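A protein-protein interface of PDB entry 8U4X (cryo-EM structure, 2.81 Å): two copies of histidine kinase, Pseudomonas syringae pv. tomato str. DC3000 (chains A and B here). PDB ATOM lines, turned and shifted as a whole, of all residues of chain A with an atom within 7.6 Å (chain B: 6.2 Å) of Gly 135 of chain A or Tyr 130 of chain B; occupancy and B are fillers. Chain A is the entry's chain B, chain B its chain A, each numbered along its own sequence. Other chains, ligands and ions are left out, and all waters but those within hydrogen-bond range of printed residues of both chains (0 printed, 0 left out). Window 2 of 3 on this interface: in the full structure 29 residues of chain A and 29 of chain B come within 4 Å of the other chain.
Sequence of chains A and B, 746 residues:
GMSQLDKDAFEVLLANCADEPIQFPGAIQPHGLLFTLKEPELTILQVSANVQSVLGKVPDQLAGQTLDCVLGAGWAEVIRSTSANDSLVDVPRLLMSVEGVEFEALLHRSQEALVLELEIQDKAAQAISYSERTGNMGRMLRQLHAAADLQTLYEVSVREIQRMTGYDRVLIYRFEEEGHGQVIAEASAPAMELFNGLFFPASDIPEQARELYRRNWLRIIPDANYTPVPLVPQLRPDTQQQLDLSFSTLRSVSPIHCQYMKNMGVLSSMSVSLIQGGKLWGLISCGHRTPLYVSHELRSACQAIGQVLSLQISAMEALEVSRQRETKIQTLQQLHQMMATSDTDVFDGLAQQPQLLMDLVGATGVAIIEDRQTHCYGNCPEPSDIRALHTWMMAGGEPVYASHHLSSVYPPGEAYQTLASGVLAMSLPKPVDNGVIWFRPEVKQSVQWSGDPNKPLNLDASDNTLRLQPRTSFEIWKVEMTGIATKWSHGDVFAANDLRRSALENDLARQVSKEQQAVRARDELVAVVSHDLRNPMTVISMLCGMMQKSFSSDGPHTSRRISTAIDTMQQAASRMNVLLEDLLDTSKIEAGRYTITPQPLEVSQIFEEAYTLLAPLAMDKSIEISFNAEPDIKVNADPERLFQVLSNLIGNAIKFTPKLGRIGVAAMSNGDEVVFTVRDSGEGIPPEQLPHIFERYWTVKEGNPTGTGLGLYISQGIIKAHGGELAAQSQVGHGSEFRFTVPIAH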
ATOM      1  N   SER A 129       2.422 -29.170  30.702  1.00  0.00           N
ATOM      2  CA  SER A 129       2.652 -29.301  29.271  1.00  0.00           C
ATOM      3  C   SER A 129       4.119 -29.050  28.955  1.00  0.00           C
ATOM      4  O   SER A 129       4.790 -28.263  29.630  1.00  0.00           O
ATOM      5  CB  SER A 129       1.770 -28.332  28.477  1.00  0.00           C
ATOM      6  OG  SER A 129       2.120 -28.333  27.103  1.00  0.00           O
ATOM      7  N   TYR A 130       4.612 -29.731  27.919  1.00  0.00           N
ATOM      8  CA  TYR A 130       6.011 -29.622  27.524  1.00  0.00           C
ATOM      9  C   TYR A 130       6.330 -28.303  26.830  1.00  0.00           C
ATOM     10  O   TYR A 130       7.509 -28.000  26.622  1.00  0.00           O
ATOM     11  CB  TYR A 130       6.377 -30.797  26.611  1.00  0.00           C
ATOM     12  CG  TYR A 130       7.856 -30.944  26.331  1.00  0.00           C
ATOM     13  CD1 TYR A 130       8.729 -31.391  27.314  1.00  0.00           C
ATOM     14  CD2 TYR A 130       8.378 -30.643  25.080  1.00  0.00           C
ATOM     15  CE1 TYR A 130      10.079 -31.533  27.060  1.00  0.00           C
ATOM     16  CE2 TYR A 130       9.728 -30.779  24.816  1.00  0.00           C
ATOM     17  CZ  TYR A 130      10.573 -31.223  25.810  1.00  0.00           C
ATOM     18  OH  TYR A 130      11.917 -31.360  25.551  1.00  0.00           O
ATOM     19  N   SER A 131       5.316 -27.511  26.475  1.00  0.00           N
ATOM     20  CA  SER A 131       5.562 -26.297  25.704  1.00  0.00           C
ATOM     21  C   SER A 131       6.069 -25.164  26.590  1.00  0.00           C
ATOM     22  O   SER A 131       7.147 -24.609  26.348  1.00  0.00           O
ATOM     23  CB  SER A 131       4.288 -25.879  24.970  1.00  0.00           C
ATOM     24  OG  SER A 131       3.683 -26.986  24.327  1.00  0.00           O
ATOM     25  N   GLU A 132       5.297 -24.800  27.618  1.00  0.00           N
ATOM     26  CA  GLU A 132       5.643 -23.634  28.428  1.00  0.00           C
ATOM     27  C   GLU A 132       6.939 -23.849  29.202  1.00  0.00           C
ATOM     28  O   GLU A 132       7.777 -22.943  29.282  1.00  0.00           O
ATOM     29  CB  GLU A 132       4.501 -23.297  29.386  1.00  0.00           C
ATOM     30  CG  GLU A 132       3.114 -23.506  28.804  1.00  0.00           C
ATOM     31  CD  GLU A 132       2.536 -24.862  29.159  1.00  0.00           C
ATOM     32  OE1 GLU A 132       3.314 -25.747  29.574  1.00  0.00           O
ATOM     33  OE2 GLU A 132       1.308 -25.042  29.025  1.00  0.00           O
ATOM     34  N   ARG A 133       7.125 -25.038  29.779  1.00  0.00           N
ATOM     35  CA  ARG A 133       8.324 -25.300  30.565  1.00  0.00           C
ATOM     36  C   ARG A 133       9.578 -25.396  29.709  1.00  0.00           C
ATOM     37  O   ARG A 133      10.685 -25.252  30.240  1.00  0.00           O
ATOM     38  CB  ARG A 133       8.147 -26.580  31.382  1.00  0.00           C
ATOM     39  CG  ARG A 133       6.734 -26.787  31.899  1.00  0.00           C
ATOM     40  CD  ARG A 133       6.731 -27.569  33.202  1.00  0.00           C
ATOM     41  NE  ARG A 133       6.463 -26.712  34.350  1.00  0.00           N
ATOM     42  CZ  ARG A 133       6.376 -27.141  35.602  1.00  0.00           C
ATOM     43  NH1 ARG A 133       6.530 -28.420  35.906  1.00  0.00           N
ATOM     44  NH2 ARG A 133       6.129 -26.267  36.572  1.00  0.00           N
ATOM     45  N   THR A 134       9.436 -25.635  28.406  1.00  0.00           N
ATOM     46  CA  THR A 134      10.562 -25.627  27.481  1.00  0.00           C
ATOM     47  C   THR A 134      10.515 -24.445  26.522  1.00  0.00           C
ATOM     48  O   THR A 134      11.243 -24.440  25.523  1.00  0.00           O
ATOM     49  CB  THR A 134      10.617 -26.939  26.696  1.00  0.00           C
ATOM     50  OG1 THR A 134       9.487 -27.024  25.819  1.00  0.00           O
ATOM     51  CG2 THR A 134      10.610 -28.126  27.646  1.00  0.00           C
ATOM     52  N   GLY A 135       9.668 -23.449  26.793  1.00  0.00           N
ATOM     53  CA  GLY A 135       9.647 -22.258  25.963  1.00  0.00           C
ATOM     54  C   GLY A 135      10.931 -21.456  26.034  1.00  0.00           C
ATOM     55  O   GLY A 135      11.352 -20.869  25.034  1.00  0.00           O
ATOM     56  N   ASN A 136      11.566 -21.420  27.204  1.00  0.00           N
ATOM     57  CA  ASN A 136      12.832 -20.729  27.397  1.00  0.00           C
ATOM     58  C   ASN A 136      14.034 -21.611  27.080  1.00  0.00           C
ATOM     59  O   ASN A 136      15.130 -21.353  27.587  1.00  0.00           O
ATOM     60  CB  ASN A 136      12.934 -20.206  28.831  1.00  0.00           C
ATOM     61  CG  ASN A 136      11.876 -19.166  29.149  1.00  0.00           C
ATOM     62  OD1 ASN A 136      10.680 -19.421  29.021  1.00  0.00           O
ATOM     63  ND2 ASN A 136      12.315 -17.985  29.569  1.00  0.00           N
ATOM     64  N   MET A 137      13.848 -22.649  26.260  1.00  0.00           N
ATOM     65  CA  MET A 137      14.950 -23.547  25.926  1.00  0.00           C
ATOM     66  C   MET A 137      16.054 -22.809  25.177  1.00  0.00           C
ATOM     67  O   MET A 137      17.220 -22.835  25.592  1.00  0.00           O
ATOM     68  CB  MET A 137      14.421 -24.716  25.094  1.00  0.00           C
ATOM     69  CG  MET A 137      15.470 -25.698  24.595  1.00  0.00           C
ATOM     70  SD  MET A 137      15.562 -27.183  25.616  1.00  0.00           S
ATOM     71  CE  MET A 137      17.157 -27.843  25.140  1.00  0.00           C
ATOM     72  N   GLY A 138      15.699 -22.117  24.091  1.00  0.00           N
ATOM     73  CA  GLY A 138      16.705 -21.424  23.302  1.00  0.00           C
ATOM     74  C   GLY A 138      17.411 -20.331  24.080  1.00  0.00           C
ATOM     75  O   GLY A 138      18.625 -20.148  23.948  1.00  0.00           O
ATOM     76  N   ARG A 139      16.663 -19.592  24.901  1.00  0.00           N
ATOM     77  CA  ARG A 139      17.286 -18.597  25.767  1.00  0.00           C
ATOM     78  C   ARG A 139      18.236 -19.257  26.756  1.00  0.00           C
ATOM     79  O   ARG A 139      19.297 -18.707  27.075  1.00  0.00           O
ATOM     80  CB  ARG A 139      16.214 -17.794  26.503  1.00  0.00           C
ATOM     81  CG  ARG A 139      15.690 -16.598  25.724  1.00  0.00           C
ATOM     82  CD  ARG A 139      15.116 -15.539  26.652  1.00  0.00           C
ATOM     83  NE  ARG A 139      16.122 -15.005  27.562  1.00  0.00           N
ATOM     84  CZ  ARG A 139      16.057 -15.091  28.884  1.00  0.00           C
ATOM     85  NH1 ARG A 139      15.044 -15.690  29.488  1.00  0.00           N
ATOM     86  NH2 ARG A 139      17.033 -14.563  29.617  1.00  0.00           N
ATOM     87  N   MET A 140      17.873 -20.443  27.250  1.00  0.00           N
ATOM     88  CA  MET A 140      18.748 -21.159  28.172  1.00  0.00           C
ATOM     89  C   MET A 140      20.053 -21.564  27.496  1.00  0.00           C
ATOM     90  O   MET A 140      21.133 -21.413  28.077  1.00  0.00           O
ATOM     91  CB  MET A 140      18.022 -22.379  28.740  1.00  0.00           C
ATOM     92  CG  MET A 140      18.931 -23.472  29.277  1.00  0.00           C
ATOM     93  SD  MET A 140      19.292 -24.737  28.046  1.00  0.00           S
ATOM     94  CE  MET A 140      17.697 -25.539  27.938  1.00  0.00           C
ATOM     95  N   ARG A 142      21.367 -20.069  24.891  1.00  0.00           N
ATOM     96  CA  ARG A 142      22.093 -18.827  24.640  1.00  0.00           C
ATOM     97  C   ARG A 142      22.829 -18.362  25.890  1.00  0.00           C
ATOM     98  O   ARG A 142      23.980 -17.918  25.813  1.00  0.00           O
ATOM     99  CB  ARG A 142      21.132 -17.747  24.145  1.00  0.00           C
ATOM    100  CG  ARG A 142      21.073 -17.612  22.632  1.00  0.00           C
ATOM    101  CD  ARG A 142      19.938 -16.696  22.203  1.00  0.00           C
ATOM    102  NE  ARG A 142      18.631 -17.311  22.402  1.00  0.00           N
ATOM    103  CZ  ARG A 142      17.477 -16.671  22.276  1.00  0.00           C
ATOM    104  NH1 ARG A 142      17.429 -15.389  21.952  1.00  0.00           N
ATOM    105  NH2 ARG A 142      16.343 -17.335  22.479  1.00  0.00           N
ATOM    106  N   GLU A 160      17.517 -23.196  35.448  1.00  0.00           N
ATOM    107  CA  GLU A 160      16.600 -23.673  34.418  1.00  0.00           C
ATOM    108  C   GLU A 160      16.006 -25.026  34.789  1.00  0.00           C
ATOM    109  O   GLU A 160      14.806 -25.262  34.590  1.00  0.00           O
ATOM    110  CB  GLU A 160      17.322 -23.751  33.073  1.00  0.00           C
ATOM    111  CG  GLU A 160      16.397 -23.829  31.869  1.00  0.00           C
ATOM    112  CD  GLU A 160      15.525 -22.598  31.718  1.00  0.00           C
ATOM    113  OE1 GLU A 160      16.070 -21.473  31.716  1.00  0.00           O
ATOM    114  OE2 GLU A 160      14.292 -22.756  31.602  1.00  0.00           O
ATOM    115  N   ARG A 163      13.450 -24.601  37.306  1.00  0.00           N
ATOM    116  CA  ARG A 163      12.289 -23.960  36.698  1.00  0.00           C
ATOM    117  C   ARG A 163      11.384 -24.979  36.019  1.00  0.00           C
ATOM    118  O   ARG A 163      10.161 -24.952  36.202  1.00  0.00           O
ATOM    119  CB  ARG A 163      12.745 -22.899  35.697  1.00  0.00           C
ATOM    120  CG  ARG A 163      11.835 -21.688  35.616  1.00  0.00           C
ATOM    121  CD  ARG A 163      12.221 -20.792  34.450  1.00  0.00           C
ATOM    122  NE  ARG A 163      12.133 -21.490  33.172  1.00  0.00           N
ATOM    123  CZ  ARG A 163      10.998 -21.767  32.545  1.00  0.00           C
ATOM    124  NH1 ARG A 163       9.825 -21.409  33.043  1.00  0.00           N
ATOM    125  NH2 ARG A 163      11.040 -22.420  31.386  1.00  0.00           N
ATOM    126  N   ARG B  93      11.526 -11.364  25.121  1.00  0.00           N
ATOM    127  CA  ARG B  93      10.723 -11.019  23.956  1.00  0.00           C
ATOM    128  C   ARG B  93       9.992  -9.701  24.178  1.00  0.00           C
ATOM    129  O   ARG B  93       9.541  -9.400  25.287  1.00  0.00           O
ATOM    130  CB  ARG B  93       9.718 -12.131  23.658  1.00  0.00           C
ATOM    131  CG  ARG B  93      10.344 -13.420  23.157  1.00  0.00           C
ATOM    132  CD  ARG B  93       9.390 -14.161  22.238  1.00  0.00           C
ATOM    133  NE  ARG B  93       9.075 -13.385  21.045  1.00  0.00           N
ATOM    134  CZ  ARG B  93       8.278 -13.799  20.069  1.00  0.00           C
ATOM    135  NH1 ARG B  93       7.694 -14.986  20.111  1.00  0.00           N
ATOM    136  NH2 ARG B  93       8.062 -13.004  19.025  1.00  0.00           N
ATOM    137  N   ILE B 128       2.551 -18.362  12.421  1.00  0.00           N
ATOM    138  CA  ILE B 128       3.639 -19.235  12.841  1.00  0.00           C
ATOM    139  C   ILE B 128       3.922 -19.011  14.319  1.00  0.00           C
ATOM    140  O   ILE B 128       4.081 -17.871  14.770  1.00  0.00           O
ATOM    141  CB  ILE B 128       4.890 -18.981  11.982  1.00  0.00           C
ATOM    142  CG1 ILE B 128       4.656 -19.455  10.546  1.00  0.00           C
ATOM    143  CG2 ILE B 128       6.107 -19.664  12.587  1.00  0.00           C
ATOM    144  CD1 ILE B 128       5.816 -19.176   9.615  1.00  0.00           C
ATOM    145  N   SER B 129       3.987 -20.101  15.079  1.00  0.00           N
ATOM    146  CA  SER B 129       4.222 -20.047  16.513  1.00  0.00           C
ATOM    147  C   SER B 129       5.531 -20.746  16.854  1.00  0.00           C
ATOM    148  O   SER B 129       5.932 -21.704  16.186  1.00  0.00           O
ATOM    149  CB  SER B 129       3.067 -20.690  17.288  1.00  0.00           C
ATOM    150  OG  SER B 129       3.377 -20.797  18.667  1.00  0.00           O
ATOM    151  N   TYR B 130       6.195 -20.252  17.900  1.00  0.00           N
ATOM    152  CA  TYR B 130       7.482 -20.793  18.318  1.00  0.00           C
ATOM    153  C   TYR B 130       7.360 -22.145  19.011  1.00  0.00           C
ATOM    154  O   TYR B 130       8.380 -22.803  19.238  1.00  0.00           O
ATOM    155  CB  TYR B 130       8.182 -19.792  19.241  1.00  0.00           C
ATOM    156  CG  TYR B 130       9.628 -20.116  19.547  1.00  0.00           C
ATOM    157  CD1 TYR B 130      10.613 -19.965  18.580  1.00  0.00           C
ATOM    158  CD2 TYR B 130      10.007 -20.563  20.806  1.00  0.00           C
ATOM    159  CE1 TYR B 130      11.935 -20.254  18.857  1.00  0.00           C
ATOM    160  CE2 TYR B 130      11.327 -20.858  21.091  1.00  0.00           C
ATOM    161  CZ  TYR B 130      12.286 -20.701  20.114  1.00  0.00           C
ATOM    162  OH  TYR B 130      13.602 -20.993  20.395  1.00  0.00           O
ATOM    163  N   SER B 131       6.143 -22.579  19.346  1.00  0.00           N
ATOM    164  CA  SER B 131       5.981 -23.808  20.116  1.00  0.00           C
ATOM    165  C   SER B 131       6.122 -25.043  19.234  1.00  0.00           C
ATOM    166  O   SER B 131       6.968 -25.908  19.491  1.00  0.00           O
ATOM    167  CB  SER B 131       4.628 -23.805  20.827  1.00  0.00           C
ATOM    168  OG  SER B 131       4.390 -22.562  21.465  1.00  0.00           O
ATOM    169  N   GLU B 132       5.293 -25.149  18.191  1.00  0.00           N
ATOM    170  CA  GLU B 132       5.271 -26.366  17.382  1.00  0.00           C
ATOM    171  C   GLU B 132       6.582 -26.568  16.631  1.00  0.00           C
ATOM    172  O   GLU B 132       7.093 -27.692  16.562  1.00  0.00           O
ATOM    173  CB  GLU B 132       4.096 -26.328  16.403  1.00  0.00           C
ATOM    174  CG  GLU B 132       2.835 -25.693  16.964  1.00  0.00           C
ATOM    175  CD  GLU B 132       2.718 -24.227  16.605  1.00  0.00           C
ATOM    176  OE1 GLU B 132       3.741 -23.630  16.208  1.00  0.00           O
ATOM    177  OE2 GLU B 132       1.606 -23.671  16.720  1.00  0.00           O
ATOM    178  N   ARG B 133       7.140 -25.498  16.063  1.00  0.00           N
ATOM    179  CA  ARG B 133       8.373 -25.626  15.297  1.00  0.00           C
ATOM    180  C   ARG B 133       9.580 -25.927  16.174  1.00  0.00           C
ATOM    181  O   ARG B 133      10.595 -26.412  15.661  1.00  0.00           O
ATOM    182  CB  ARG B 133       8.622 -24.356  14.482  1.00  0.00           C
ATOM    183  CG  ARG B 133       7.354 -23.717  13.943  1.00  0.00           C
ATOM    184  CD  ARG B 133       7.618 -22.976  12.644  1.00  0.00           C
ATOM    185  NE  ARG B 133       7.114 -23.707  11.487  1.00  0.00           N
ATOM    186  CZ  ARG B 133       7.189 -23.273  10.237  1.00  0.00           C
ATOM    187  NH1 ARG B 133       7.741 -22.108   9.941  1.00  0.00           N
ATOM    188  NH2 ARG B 133       6.696 -24.028   9.258  1.00  0.00           N
ATOM    189  N   THR B 134       9.499 -25.656  17.476  1.00  0.00           N
ATOM    190  CA  THR B 134      10.549 -26.013  18.419  1.00  0.00           C
ATOM    191  C   THR B 134      10.117 -27.120  19.373  1.00  0.00           C
ATOM    192  O   THR B 134      10.789 -27.352  20.382  1.00  0.00           O
ATOM    193  CB  THR B 134      10.999 -24.785  19.210  1.00  0.00           C
ATOM    194  OG1 THR B 134       9.938 -24.349  20.069  1.00  0.00           O
ATOM    195  CG2 THR B 134      11.381 -23.657  18.265  1.00  0.00           C
ATOM    196  N   GLY B 135       9.006 -27.800  19.083  1.00  0.00           N
ATOM    197  CA  GLY B 135       8.597 -28.925  19.907  1.00  0.00           C
ATOM    198  C   GLY B 135       9.567 -30.089  19.855  1.00  0.00           C
ATOM    199  O   GLY B 135       9.765 -30.777  20.860  1.00  0.00           O
ATOM    200  N   MET B 137      12.714 -29.871  19.682  1.00  0.00           N
ATOM    201  CA  MET B 137      14.036 -29.364  20.037  1.00  0.00           C
ATOM    202  C   MET B 137      14.840 -30.410  20.803  1.00  0.00           C
ATOM    203  O   MET B 137      15.962 -30.751  20.407  1.00  0.00           O
ATOM    204  CB  MET B 137      13.885 -28.087  20.867  1.00  0.00           C
ATOM    205  CG  MET B 137      15.181 -27.483  21.387  1.00  0.00           C
ATOM    206  SD  MET B 137      15.752 -26.102  20.373  1.00  0.00           S
ATOM    207  CE  MET B 137      17.465 -25.976  20.879  1.00  0.00           C
ATOM    208  N   MET B 164      12.089 -26.220  10.703  1.00  0.00           N
ATOM    209  CA  MET B 164      11.579 -25.037  11.394  1.00  0.00           C
ATOM    210  C   MET B 164      11.452 -23.855  10.440  1.00  0.00           C
ATOM    211  O   MET B 164      10.445 -23.136  10.450  1.00  0.00           O
ATOM    212  CB  MET B 164      12.470 -24.659  12.577  1.00  0.00           C
ATOM    213  CG  MET B 164      13.922 -25.019  12.432  1.00  0.00           C
ATOM    214  SD  MET B 164      14.727 -25.107  14.036  1.00  0.00           S
ATOM    215  CE  MET B 164      14.268 -23.519  14.711  1.00  0.00           C
ATOM    216  N   GLU B 297      12.581 -15.194  16.743  1.00  0.00           N
ATOM    217  CA  GLU B 297      12.686 -16.304  17.685  1.00  0.00           C
ATOM    218  C   GLU B 297      13.221 -17.558  17.005  1.00  0.00           C
ATOM    219  O   GLU B 297      14.108 -18.236  17.542  1.00  0.00           O
ATOM    220  CB  GLU B 297      11.326 -16.576  18.325  1.00  0.00           C
ATOM    221  CG  GLU B 297      11.169 -15.980  19.711  1.00  0.00           C
ATOM    222  CD  GLU B 297      12.254 -16.438  20.664  1.00  0.00           C
ATOM    223  OE1 GLU B 297      12.350 -17.657  20.915  1.00  0.00           O
ATOM    224  OE2 GLU B 297      13.013 -15.580  21.162  1.00  0.00           O
ATOM    225  N   LEU B 298      12.706 -17.876  15.816  1.00  0.00           N
ATOM    226  CA  LEU B 298      13.212 -19.032  15.083  1.00  0.00           C
ATOM    227  C   LEU B 298      14.655 -18.815  14.645  1.00  0.00           C
ATOM    228  O   LEU B 298      15.447 -19.763  14.611  1.00  0.00           O
ATOM    229  CB  LEU B 298      12.319 -19.324  13.877  1.00  0.00           C
ATOM    230  CG  LEU B 298      10.881 -19.747  14.188  1.00  0.00           C
ATOM    231  CD1 LEU B 298       9.888 -18.736  13.636  1.00  0.00           C
ATOM    232  CD2 LEU B 298      10.601 -21.137  13.639  1.00  0.00           C
ATOM    233  N   ARG B 299      15.016 -17.575  14.309  1.00  0.00           N
ATOM    234  CA  ARG B 299      16.399 -17.283  13.944  1.00  0.00           C
ATOM    235  C   ARG B 299      17.338 -17.493  15.126  1.00  0.00           C
ATOM    236  O   ARG B 299      18.434 -18.041  14.968  1.00  0.00           O
ATOM    237  CB  ARG B 299      16.505 -15.855  13.413  1.00  0.00           C
ATOM    238  CG  ARG B 299      15.625 -15.579  12.209  1.00  0.00           C
ATOM    239  CD  ARG B 299      16.131 -14.388  11.419  1.00  0.00           C
ATOM    240  NE  ARG B 299      16.251 -13.203  12.258  1.00  0.00           N
ATOM    241  CZ  ARG B 299      15.471 -12.136  12.158  1.00  0.00           C
ATOM    242  NH1 ARG B 299      14.491 -12.075  11.272  1.00  0.00           N
ATOM    243  NH2 ARG B 299      15.678 -11.104  12.972  1.00  0.00           N
ATOM    244  N   SER B 300      16.924 -17.066  16.324  1.00  0.00           N
ATOM    245  CA  SER B 300      17.726 -17.302  17.520  1.00  0.00           C
ATOM    246  C   SER B 300      17.826 -18.788  17.842  1.00  0.00           C
ATOM    247  O   SER B 300      18.887 -19.269  18.262  1.00  0.00           O
ATOM    248  CB  SER B 300      17.139 -16.536  18.706  1.00  0.00           C
ATOM    249  OG  SER B 300      16.568 -15.307  18.292  1.00  0.00           O
ATOM    250  N   ALA B 301      16.731 -19.531  17.659  1.00  0.00           N
ATOM    251  CA  ALA B 301      16.782 -20.976  17.859  1.00  0.00           C
ATOM    252  C   ALA B 301      17.755 -21.630  16.885  1.00  0.00           C
ATOM    253  O   ALA B 301      18.522 -22.522  17.264  1.00  0.00           O
ATOM    254  CB  ALA B 301      15.387 -21.578  17.709  1.00  0.00           C
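OE2 of Glu 297 of chain B is in salt-bridge range of NH2 of Arg 142 of chain A (3.99 Å).
Tyr 130 of chain A touches Gly 135 of chain B. O of Gly 135 of chain A touches CE2 of Tyr 130 of chain B (3.9 Å). Met 137 of chain B touches Met 137 of chain A (CG to CG, 3.7 Å). Arg 142 of chain A touches Ser 300 of chain B.
The backbone carbonyl oxygen (O) of Gly 138 of chain A is in hydrogen-bond range of the guanidinium group (NE) of Arg 142 of chain A, 3.2 Å away.
Of the 15 printed residues of chain A, 4 touch a printed residue of chain B. Printed residues of chain B that touch a printed residue of chain A: Tyr 130, Gly 135, Met 137, Glu 297 and Ser 300. Hydrophobic or aromatic side chains of chain B within 4 Å of the printed part of chain A: Tyr 130 and Met 137. Among the printed residues, 5 pairs touch across the chains. Among the printed residues, Asp or Glu carboxylates within 4 Å of a Lys or Arg side-chain nitrogen of the other chain: Arg 142 of chain A with Glu 297 of chain B.
Tyr 130 of chain A touches Gly 135 of chain B, and with the chains exchanged Gly 135 of chain A touches Tyr 130 of chain B. Met 137 of chain B touches its own counterpart, Met 137 of chain A. Positions printed for both chains: 129, 130, 131, 132, 133, 134, 135 and 137. Of the 5 pairs that touch across the chains among the printed residues, 3 have their exchanged pair printed and touching as well.
Printed residues of chain B within 4 Å of Tyr 130 of chain A: Gly 135 (3.96 Å). Gly 135 of chain A touches one residue of chain B. Of chain A, only Gly 135 comes within 4 Å of Tyr 130 of chain B. Of the printed residues of chain A, Gly 135 of chain B touches Tyr 130 (3.96 Å). Of the printed residues of chain A, Met 137 of chain B touches Met 137 (3.7 Å). The nearest residue of chain B that does not touch Gly 135 of chain A is Glu 297 of chain B (5.3 Å). The nearest printed residue of chain A that does not touch Met 137 of chain B is Gly 138 of chain A (5.2 Å).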
